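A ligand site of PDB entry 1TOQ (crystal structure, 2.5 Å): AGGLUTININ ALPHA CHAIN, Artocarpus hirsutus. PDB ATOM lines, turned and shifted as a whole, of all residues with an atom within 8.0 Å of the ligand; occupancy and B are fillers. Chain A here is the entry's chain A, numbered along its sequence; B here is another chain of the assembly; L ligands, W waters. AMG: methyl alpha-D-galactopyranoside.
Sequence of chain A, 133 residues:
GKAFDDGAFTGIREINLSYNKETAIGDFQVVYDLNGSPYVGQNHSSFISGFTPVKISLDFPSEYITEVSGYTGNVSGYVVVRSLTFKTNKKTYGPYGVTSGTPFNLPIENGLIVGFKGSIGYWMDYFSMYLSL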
ATOM      1  N   GLY A   1       4.659   9.660 -12.057  1.00  0.00           N
ATOM      2  CA  GLY A   1       4.625   8.790 -10.836  1.00  0.00           C
ATOM      3  C   GLY A   1       3.676   7.639 -11.157  1.00  0.00           C
ATOM      4  O   GLY A   1       3.133   7.646 -12.240  1.00  0.00           O
ATOM      5  N   LYS A   2       3.498   6.680 -10.289  1.00  0.00           N
ATOM      6  CA  LYS A   2       2.627   5.541 -10.574  1.00  0.00           C
ATOM      7  C   LYS A   2       1.265   5.821  -9.953  1.00  0.00           C
ATOM      8  O   LYS A   2       1.138   6.149  -8.762  1.00  0.00           O
ATOM      9  CB  LYS A   2       3.340   4.318 -10.027  1.00  0.00           C
ATOM     10  CG  LYS A   2       2.627   2.984 -10.219  1.00  0.00           C
ATOM     11  CD  LYS A   2       3.312   1.967  -9.303  1.00  0.00           C
ATOM     12  CE  LYS A   2       2.390   0.767  -9.059  1.00  0.00           C
ATOM     13  NZ  LYS A   2       2.684   0.079  -7.720  1.00  0.00           N
ATOM     14  N   ALA A  24       8.620  16.548   0.621  1.00  0.00           N
ATOM     15  CA  ALA A  24       7.200  16.333   0.614  1.00  0.00           C
ATOM     16  C   ALA A  24       6.782  14.977   1.167  1.00  0.00           C
ATOM     17  O   ALA A  24       7.568  14.255   1.755  1.00  0.00           O
ATOM     18  CB  ALA A  24       6.840  16.344  -0.900  1.00  0.00           C
ATOM     19  N   ILE A  25       5.536  14.599   0.864  1.00  0.00           N
ATOM     20  CA  ILE A  25       4.991  13.325   1.282  1.00  0.00           C
ATOM     21  C   ILE A  25       5.531  12.223   0.370  1.00  0.00           C
ATOM     22  O   ILE A  25       5.587  12.396  -0.856  1.00  0.00           O
ATOM     23  CB  ILE A  25       3.457  13.380   1.213  1.00  0.00           C
ATOM     24  CG1 ILE A  25       2.906  14.512   2.073  1.00  0.00           C
ATOM     25  CG2 ILE A  25       2.837  12.046   1.596  1.00  0.00           C
ATOM     26  CD1 ILE A  25       3.063  14.344   3.574  1.00  0.00           C
ATOM     27  N   SER A  46       7.011   5.459  -2.381  1.00  0.00           N
ATOM     28  CA  SER A  46       7.757   6.458  -3.160  1.00  0.00           C
ATOM     29  C   SER A  46       8.844   5.747  -3.969  1.00  0.00           C
ATOM     30  O   SER A  46       9.351   4.727  -3.503  1.00  0.00           O
ATOM     31  CB  SER A  46       8.435   7.393  -2.163  1.00  0.00           C
ATOM     32  OG  SER A  46       9.607   7.963  -2.676  1.00  0.00           O
ATOM     33  N   PHE A  47       9.300   6.265  -5.084  1.00  0.00           N
ATOM     34  CA  PHE A  47      10.402   5.671  -5.830  1.00  0.00           C
ATOM     35  C   PHE A  47      11.733   5.776  -5.069  1.00  0.00           C
ATOM     36  O   PHE A  47      12.658   5.116  -5.500  1.00  0.00           O
ATOM     37  CB  PHE A  47      10.621   6.374  -7.177  1.00  0.00           C
ATOM     38  CG  PHE A  47       9.487   6.232  -8.159  1.00  0.00           C
ATOM     39  CD1 PHE A  47       8.413   5.385  -7.934  1.00  0.00           C
ATOM     40  CD2 PHE A  47       9.519   6.967  -9.327  1.00  0.00           C
ATOM     41  CE1 PHE A  47       7.406   5.232  -8.851  1.00  0.00           C
ATOM     42  CE2 PHE A  47       8.490   6.837 -10.237  1.00  0.00           C
ATOM     43  CZ  PHE A  47       7.438   5.966 -10.020  1.00  0.00           C
ATOM     44  N   ILE A  48      11.891   6.601  -4.060  1.00  0.00           N
ATOM     45  CA  ILE A  48      13.115   6.775  -3.319  1.00  0.00           C
ATOM     46  C   ILE A  48      12.884   6.521  -1.832  1.00  0.00           C
ATOM     47  O   ILE A  48      11.759   6.223  -1.451  1.00  0.00           O
ATOM     48  CB  ILE A  48      13.742   8.184  -3.421  1.00  0.00           C
ATOM     49  CG1 ILE A  48      12.800   9.267  -2.909  1.00  0.00           C
ATOM     50  CG2 ILE A  48      14.153   8.454  -4.851  1.00  0.00           C
ATOM     51  CD1 ILE A  48      13.332  10.682  -2.926  1.00  0.00           C
ATOM     52  N   VAL A  75       8.564  20.904  -6.110  1.00  0.00           N
ATOM     53  CA  VAL A  75       9.732  20.224  -5.562  1.00  0.00           C
ATOM     54  C   VAL A  75      10.486  19.627  -6.755  1.00  0.00           C
ATOM     55  O   VAL A  75       9.932  18.836  -7.517  1.00  0.00           O
ATOM     56  CB  VAL A  75       9.475  19.126  -4.534  1.00  0.00           C
ATOM     57  CG1 VAL A  75      10.840  18.519  -4.200  1.00  0.00           C
ATOM     58  CG2 VAL A  75       8.813  19.570  -3.239  1.00  0.00           C
ATOM     59  N   SER A  76      11.693  20.130  -6.985  1.00  0.00           N
ATOM     60  CA  SER A  76      12.568  19.803  -8.080  1.00  0.00           C
ATOM     61  C   SER A  76      11.856  19.946  -9.410  1.00  0.00           C
ATOM     62  O   SER A  76      12.076  19.079 -10.275  1.00  0.00           O
ATOM     63  CB  SER A  76      13.168  18.398  -8.035  1.00  0.00           C
ATOM     64  OG  SER A  76      13.961  18.118  -6.908  1.00  0.00           O
ATOM     65  N   GLY A  77      10.999  20.936  -9.618  1.00  0.00           N
ATOM     66  CA  GLY A  77      10.280  21.085 -10.883  1.00  0.00           C
ATOM     67  C   GLY A  77       8.917  20.436 -10.888  1.00  0.00           C
ATOM     68  O   GLY A  77       8.133  20.586 -11.847  1.00  0.00           O
ATOM     69  N   TYR A  78       8.597  19.633  -9.868  1.00  0.00           N
ATOM     70  CA  TYR A  78       7.291  18.963  -9.858  1.00  0.00           C
ATOM     71  C   TYR A  78       6.324  19.561  -8.831  1.00  0.00           C
ATOM     72  O   TYR A  78       6.758  19.900  -7.727  1.00  0.00           O
ATOM     73  CB  TYR A  78       7.500  17.488  -9.501  1.00  0.00           C
ATOM     74  CG  TYR A  78       8.356  16.782 -10.514  1.00  0.00           C
ATOM     75  CD1 TYR A  78       7.769  16.306 -11.687  1.00  0.00           C
ATOM     76  CD2 TYR A  78       9.723  16.596 -10.318  1.00  0.00           C
ATOM     77  CE1 TYR A  78       8.528  15.650 -12.628  1.00  0.00           C
ATOM     78  CE2 TYR A  78      10.489  15.928 -11.256  1.00  0.00           C
ATOM     79  CZ  TYR A  78       9.882  15.474 -12.398  1.00  0.00           C
ATOM     80  OH  TYR A  78      10.623  14.826 -13.364  1.00  0.00           O
ATOM     81  N   VAL A  79       5.062  19.712  -9.236  1.00  0.00           N
ATOM     82  CA  VAL A  79       4.060  20.163  -8.280  1.00  0.00           C
ATOM     83  C   VAL A  79       3.699  18.906  -7.489  1.00  0.00           C
ATOM     84  O   VAL A  79       3.317  17.920  -8.129  1.00  0.00           O
ATOM     85  CB  VAL A  79       2.781  20.677  -8.961  1.00  0.00           C
ATOM     86  CG1 VAL A  79       1.641  20.874  -7.982  1.00  0.00           C
ATOM     87  CG2 VAL A  79       3.103  21.980  -9.692  1.00  0.00           C
ATOM     88  N   VAL A  80       3.877  18.870  -6.177  1.00  0.00           N
ATOM     89  CA  VAL A  80       3.534  17.680  -5.418  1.00  0.00           C
ATOM     90  C   VAL A  80       2.792  18.075  -4.141  1.00  0.00           C
ATOM     91  O   VAL A  80       2.712  19.265  -3.816  1.00  0.00           O
ATOM     92  CB  VAL A  80       4.815  16.920  -5.023  1.00  0.00           C
ATOM     93  CG1 VAL A  80       5.534  16.305  -6.211  1.00  0.00           C
ATOM     94  CG2 VAL A  80       5.745  17.804  -4.226  1.00  0.00           C
ATOM     95  N   VAL A  81       2.374  17.097  -3.369  1.00  0.00           N
ATOM     96  CA  VAL A  81       1.703  17.316  -2.086  1.00  0.00           C
ATOM     97  C   VAL A  81       2.785  17.331  -1.041  1.00  0.00           C
ATOM     98  O   VAL A  81       3.411  16.317  -0.699  1.00  0.00           O
ATOM     99  CB  VAL A  81       0.633  16.258  -1.789  1.00  0.00           C
ATOM    100  CG1 VAL A  81      -0.016  16.455  -0.419  1.00  0.00           C
ATOM    101  CG2 VAL A  81      -0.460  16.276  -2.872  1.00  0.00           C
ATOM    102  N   SER A 119      -1.343   9.527  -6.996  1.00  0.00           N
ATOM    103  CA  SER A 119      -0.165   9.076  -7.714  1.00  0.00           C
ATOM    104  C   SER A 119       1.066   9.403  -6.913  1.00  0.00           C
ATOM    105  O   SER A 119       1.083  10.443  -6.251  1.00  0.00           O
ATOM    106  CB  SER A 119      -0.149   9.794  -9.083  1.00  0.00           C
ATOM    107  OG  SER A 119       1.146   9.635  -9.644  1.00  0.00           O
ATOM    108  N   ILE A 120       2.025   8.501  -6.888  1.00  0.00           N
ATOM    109  CA  ILE A 120       3.266   8.707  -6.149  1.00  0.00           C
ATOM    110  C   ILE A 120       4.458   8.360  -7.056  1.00  0.00           C
ATOM    111  O   ILE A 120       4.494   7.293  -7.679  1.00  0.00           O
ATOM    112  CB  ILE A 120       3.358   7.846  -4.877  1.00  0.00           C
ATOM    113  CG1 ILE A 120       2.142   8.128  -3.982  1.00  0.00           C
ATOM    114  CG2 ILE A 120       4.652   8.125  -4.135  1.00  0.00           C
ATOM    115  CD1 ILE A 120       2.016   7.386  -2.689  1.00  0.00           C
ATOM    116  N   GLY A 121       5.398   9.275  -7.162  1.00  0.00           N
ATOM    117  CA  GLY A 121       6.632   8.984  -7.952  1.00  0.00           C
ATOM    118  C   GLY A 121       7.739   9.168  -6.916  1.00  0.00           C
ATOM    119  O   GLY A 121       7.707   8.462  -5.910  1.00  0.00           O
ATOM    120  N   TYR A 122       8.596  10.166  -7.069  1.00  0.00           N
ATOM    121  CA  TYR A 122       9.511  10.436  -5.944  1.00  0.00           C
ATOM    122  C   TYR A 122       8.618  10.858  -4.773  1.00  0.00           C
ATOM    123  O   TYR A 122       8.837  10.417  -3.650  1.00  0.00           O
ATOM    124  CB  TYR A 122      10.541  11.504  -6.244  1.00  0.00           C
ATOM    125  CG  TYR A 122      11.814  11.032  -6.925  1.00  0.00           C
ATOM    126  CD1 TYR A 122      11.812  10.029  -7.867  1.00  0.00           C
ATOM    127  CD2 TYR A 122      13.023  11.657  -6.617  1.00  0.00           C
ATOM    128  CE1 TYR A 122      12.976   9.607  -8.483  1.00  0.00           C
ATOM    129  CE2 TYR A 122      14.192  11.247  -7.228  1.00  0.00           C
ATOM    130  CZ  TYR A 122      14.158  10.225  -8.144  1.00  0.00           C
ATOM    131  OH  TYR A 122      15.329   9.857  -8.760  1.00  0.00           O
ATOM    132  N   TRP A 123       7.651  11.770  -5.013  1.00  0.00           N
ATOM    133  CA  TRP A 123       6.767  12.253  -3.968  1.00  0.00           C
ATOM    134  C   TRP A 123       5.311  12.080  -4.376  1.00  0.00           C
ATOM    135  O   TRP A 123       5.096  11.721  -5.536  1.00  0.00           O
ATOM    136  CB  TRP A 123       7.059  13.716  -3.615  1.00  0.00           C
ATOM    137  CG  TRP A 123       8.521  13.958  -3.328  1.00  0.00           C
ATOM    138  CD1 TRP A 123       9.189  13.707  -2.175  1.00  0.00           C
ATOM    139  CD2 TRP A 123       9.497  14.458  -4.259  1.00  0.00           C
ATOM    140  NE1 TRP A 123      10.525  14.023  -2.322  1.00  0.00           N
ATOM    141  CE2 TRP A 123      10.732  14.482  -3.595  1.00  0.00           C
ATOM    142  CE3 TRP A 123       9.428  14.888  -5.596  1.00  0.00           C
ATOM    143  CZ2 TRP A 123      11.908  14.936  -4.201  1.00  0.00           C
ATOM    144  CZ3 TRP A 123      10.586  15.333  -6.200  1.00  0.00           C
ATOM    145  CH2 TRP A 123      11.810  15.343  -5.503  1.00  0.00           C
ATOM    146  N   MET A 124       4.349  12.244  -3.480  1.00  0.00           N
ATOM    147  CA  MET A 124       2.942  12.166  -3.825  1.00  0.00           C
ATOM    148  C   MET A 124       2.613  13.261  -4.836  1.00  0.00           C
ATOM    149  O   MET A 124       2.762  14.460  -4.545  1.00  0.00           O
ATOM    150  CB  MET A 124       2.058  12.411  -2.590  1.00  0.00           C
ATOM    151  CG  MET A 124       0.566  12.291  -2.889  1.00  0.00           C
ATOM    152  SD  MET A 124      -0.442  12.335  -1.389  1.00  0.00           S
ATOM    153  CE  MET A 124      -0.220  10.636  -0.853  1.00  0.00           C
ATOM    154  N   ASP A 125       2.258  12.917  -6.054  1.00  0.00           N
ATOM    155  CA  ASP A 125       2.002  13.890  -7.081  1.00  0.00           C
ATOM    156  C   ASP A 125       0.659  14.599  -6.892  1.00  0.00           C
ATOM    157  O   ASP A 125       0.504  15.796  -7.157  1.00  0.00           O
ATOM    158  CB  ASP A 125       2.009  13.225  -8.461  1.00  0.00           C
ATOM    159  CG  ASP A 125       3.326  12.508  -8.714  1.00  0.00           C
ATOM    160  OD1 ASP A 125       4.397  13.125  -8.546  1.00  0.00           O
ATOM    161  OD2 ASP A 125       3.213  11.313  -9.063  1.00  0.00           O
ATOM    162  N   TYR A 126      -0.345  13.794  -6.568  1.00  0.00           N
ATOM    163  CA  TYR A 126      -1.674  14.286  -6.349  1.00  0.00           C
ATOM    164  C   TYR A 126      -2.507  13.226  -5.614  1.00  0.00           C
ATOM    165  O   TYR A 126      -2.091  12.080  -5.504  1.00  0.00           O
ATOM    166  CB  TYR A 126      -2.397  14.632  -7.646  1.00  0.00           C
ATOM    167  CG  TYR A 126      -2.496  13.536  -8.668  1.00  0.00           C
ATOM    168  CD1 TYR A 126      -3.488  12.586  -8.582  1.00  0.00           C
ATOM    169  CD2 TYR A 126      -1.629  13.425  -9.749  1.00  0.00           C
ATOM    170  CE1 TYR A 126      -3.634  11.562  -9.493  1.00  0.00           C
ATOM    171  CE2 TYR A 126      -1.745  12.420 -10.708  1.00  0.00           C
ATOM    172  CZ  TYR A 126      -2.754  11.500 -10.543  1.00  0.00           C
ATOM    173  OH  TYR A 126      -2.933  10.474 -11.453  1.00  0.00           O
ATOM    174  N   ALA B  17      -0.426  17.739  -8.647  1.00  0.00           N
ATOM    175  CA  ALA B  17      -0.044  17.986 -10.042  1.00  0.00           C
ATOM    176  C   ALA B  17      -1.297  17.842 -10.886  1.00  0.00           C
ATOM    177  O   ALA B  17      -2.222  17.134 -10.520  1.00  0.00           O
ATOM    178  CB  ALA B  17       1.109  17.125 -10.479  1.00  0.00           C
HETATM  179  C1  AMG L   1       9.642  11.231 -10.507  1.00  0.00           C
HETATM  180  C2  AMG L   1       8.629  10.812 -11.587  1.00  0.00           C
HETATM  181  C3  AMG L   1       7.774  12.021 -12.053  1.00  0.00           C
HETATM  182  C4  AMG L   1       7.131  12.672 -10.829  1.00  0.00           C
HETATM  183  C5  AMG L   1       8.222  13.053  -9.833  1.00  0.00           C
HETATM  184  C6  AMG L   1       7.686  13.680  -8.579  1.00  0.00           C
HETATM  185  C7  AMG L   1      11.600  12.552 -10.294  1.00  0.00           C
HETATM  186  O1  AMG L   1      10.547  12.112 -11.133  1.00  0.00           O
HETATM  187  O2  AMG L   1       9.428  10.449 -12.717  1.00  0.00           O
HETATM  188  O3  AMG L   1       6.751  11.539 -12.924  1.00  0.00           O
HETATM  189  O4  AMG L   1       6.347  11.666 -10.203  1.00  0.00           O
HETATM  190  O5  AMG L   1       8.926  11.854  -9.446  1.00  0.00           O
HETATM  191  O6  AMG L   1       7.079  12.732  -7.745  1.00  0.00           O
HETATM  192  O   HOH W   1       7.524   8.443 -13.916  1.00  0.00           O
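Tyr 78 touches the ligand (OH to O1, 3.5 Å). Gly 121 touches the ligand. Hydrophobic or aromatic side chains within 4 Å of the ligand: Tyr 78, Tyr 122 and Trp 123. Of the 23 residues printed, 6 come within 4 Å of the ligand. The nearest printed residue that does not touch the ligand is Val 80 (4.1 Å).
N of Tyr 122 lies within hydrogen-bond range of O5 of the ligand (2.9 Å). The backbone NH of Gly 1 sits at hydrogen-bond distance from an oxygen (O3) of the ligand (2.9 Å). The backbone carbonyl oxygen of Trp 123 is in hydrogen-bond range of an oxygen (O6) of the ligand (3.1 Å). O6 of the ligand sits at hydrogen-bond distance from OD1 of Asp 125 (2.8 Å). An oxygen (O6) of the ligand lies within hydrogen-bond range of the backbone NH of Trp 123, at 3.0 Å.
The backbone carbonyl oxygen of Tyr 122 lies within hydrogen-bond range of the side-chain hydroxyl of Ser 46 (2.8 Å). O of Asp 125 lies within hydrogen-bond range of N of Ala 17 of chain B, 2.6 Å away. O of Gly 121 sits at hydrogen-bond distance from N of Phe 47, at 2.8 Å. The side-chain carboxylate (OD2) of Asp 125 is in hydrogen-bond range of the side-chain hydroxyl (OG) of Ser 119 (2.7 Å).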
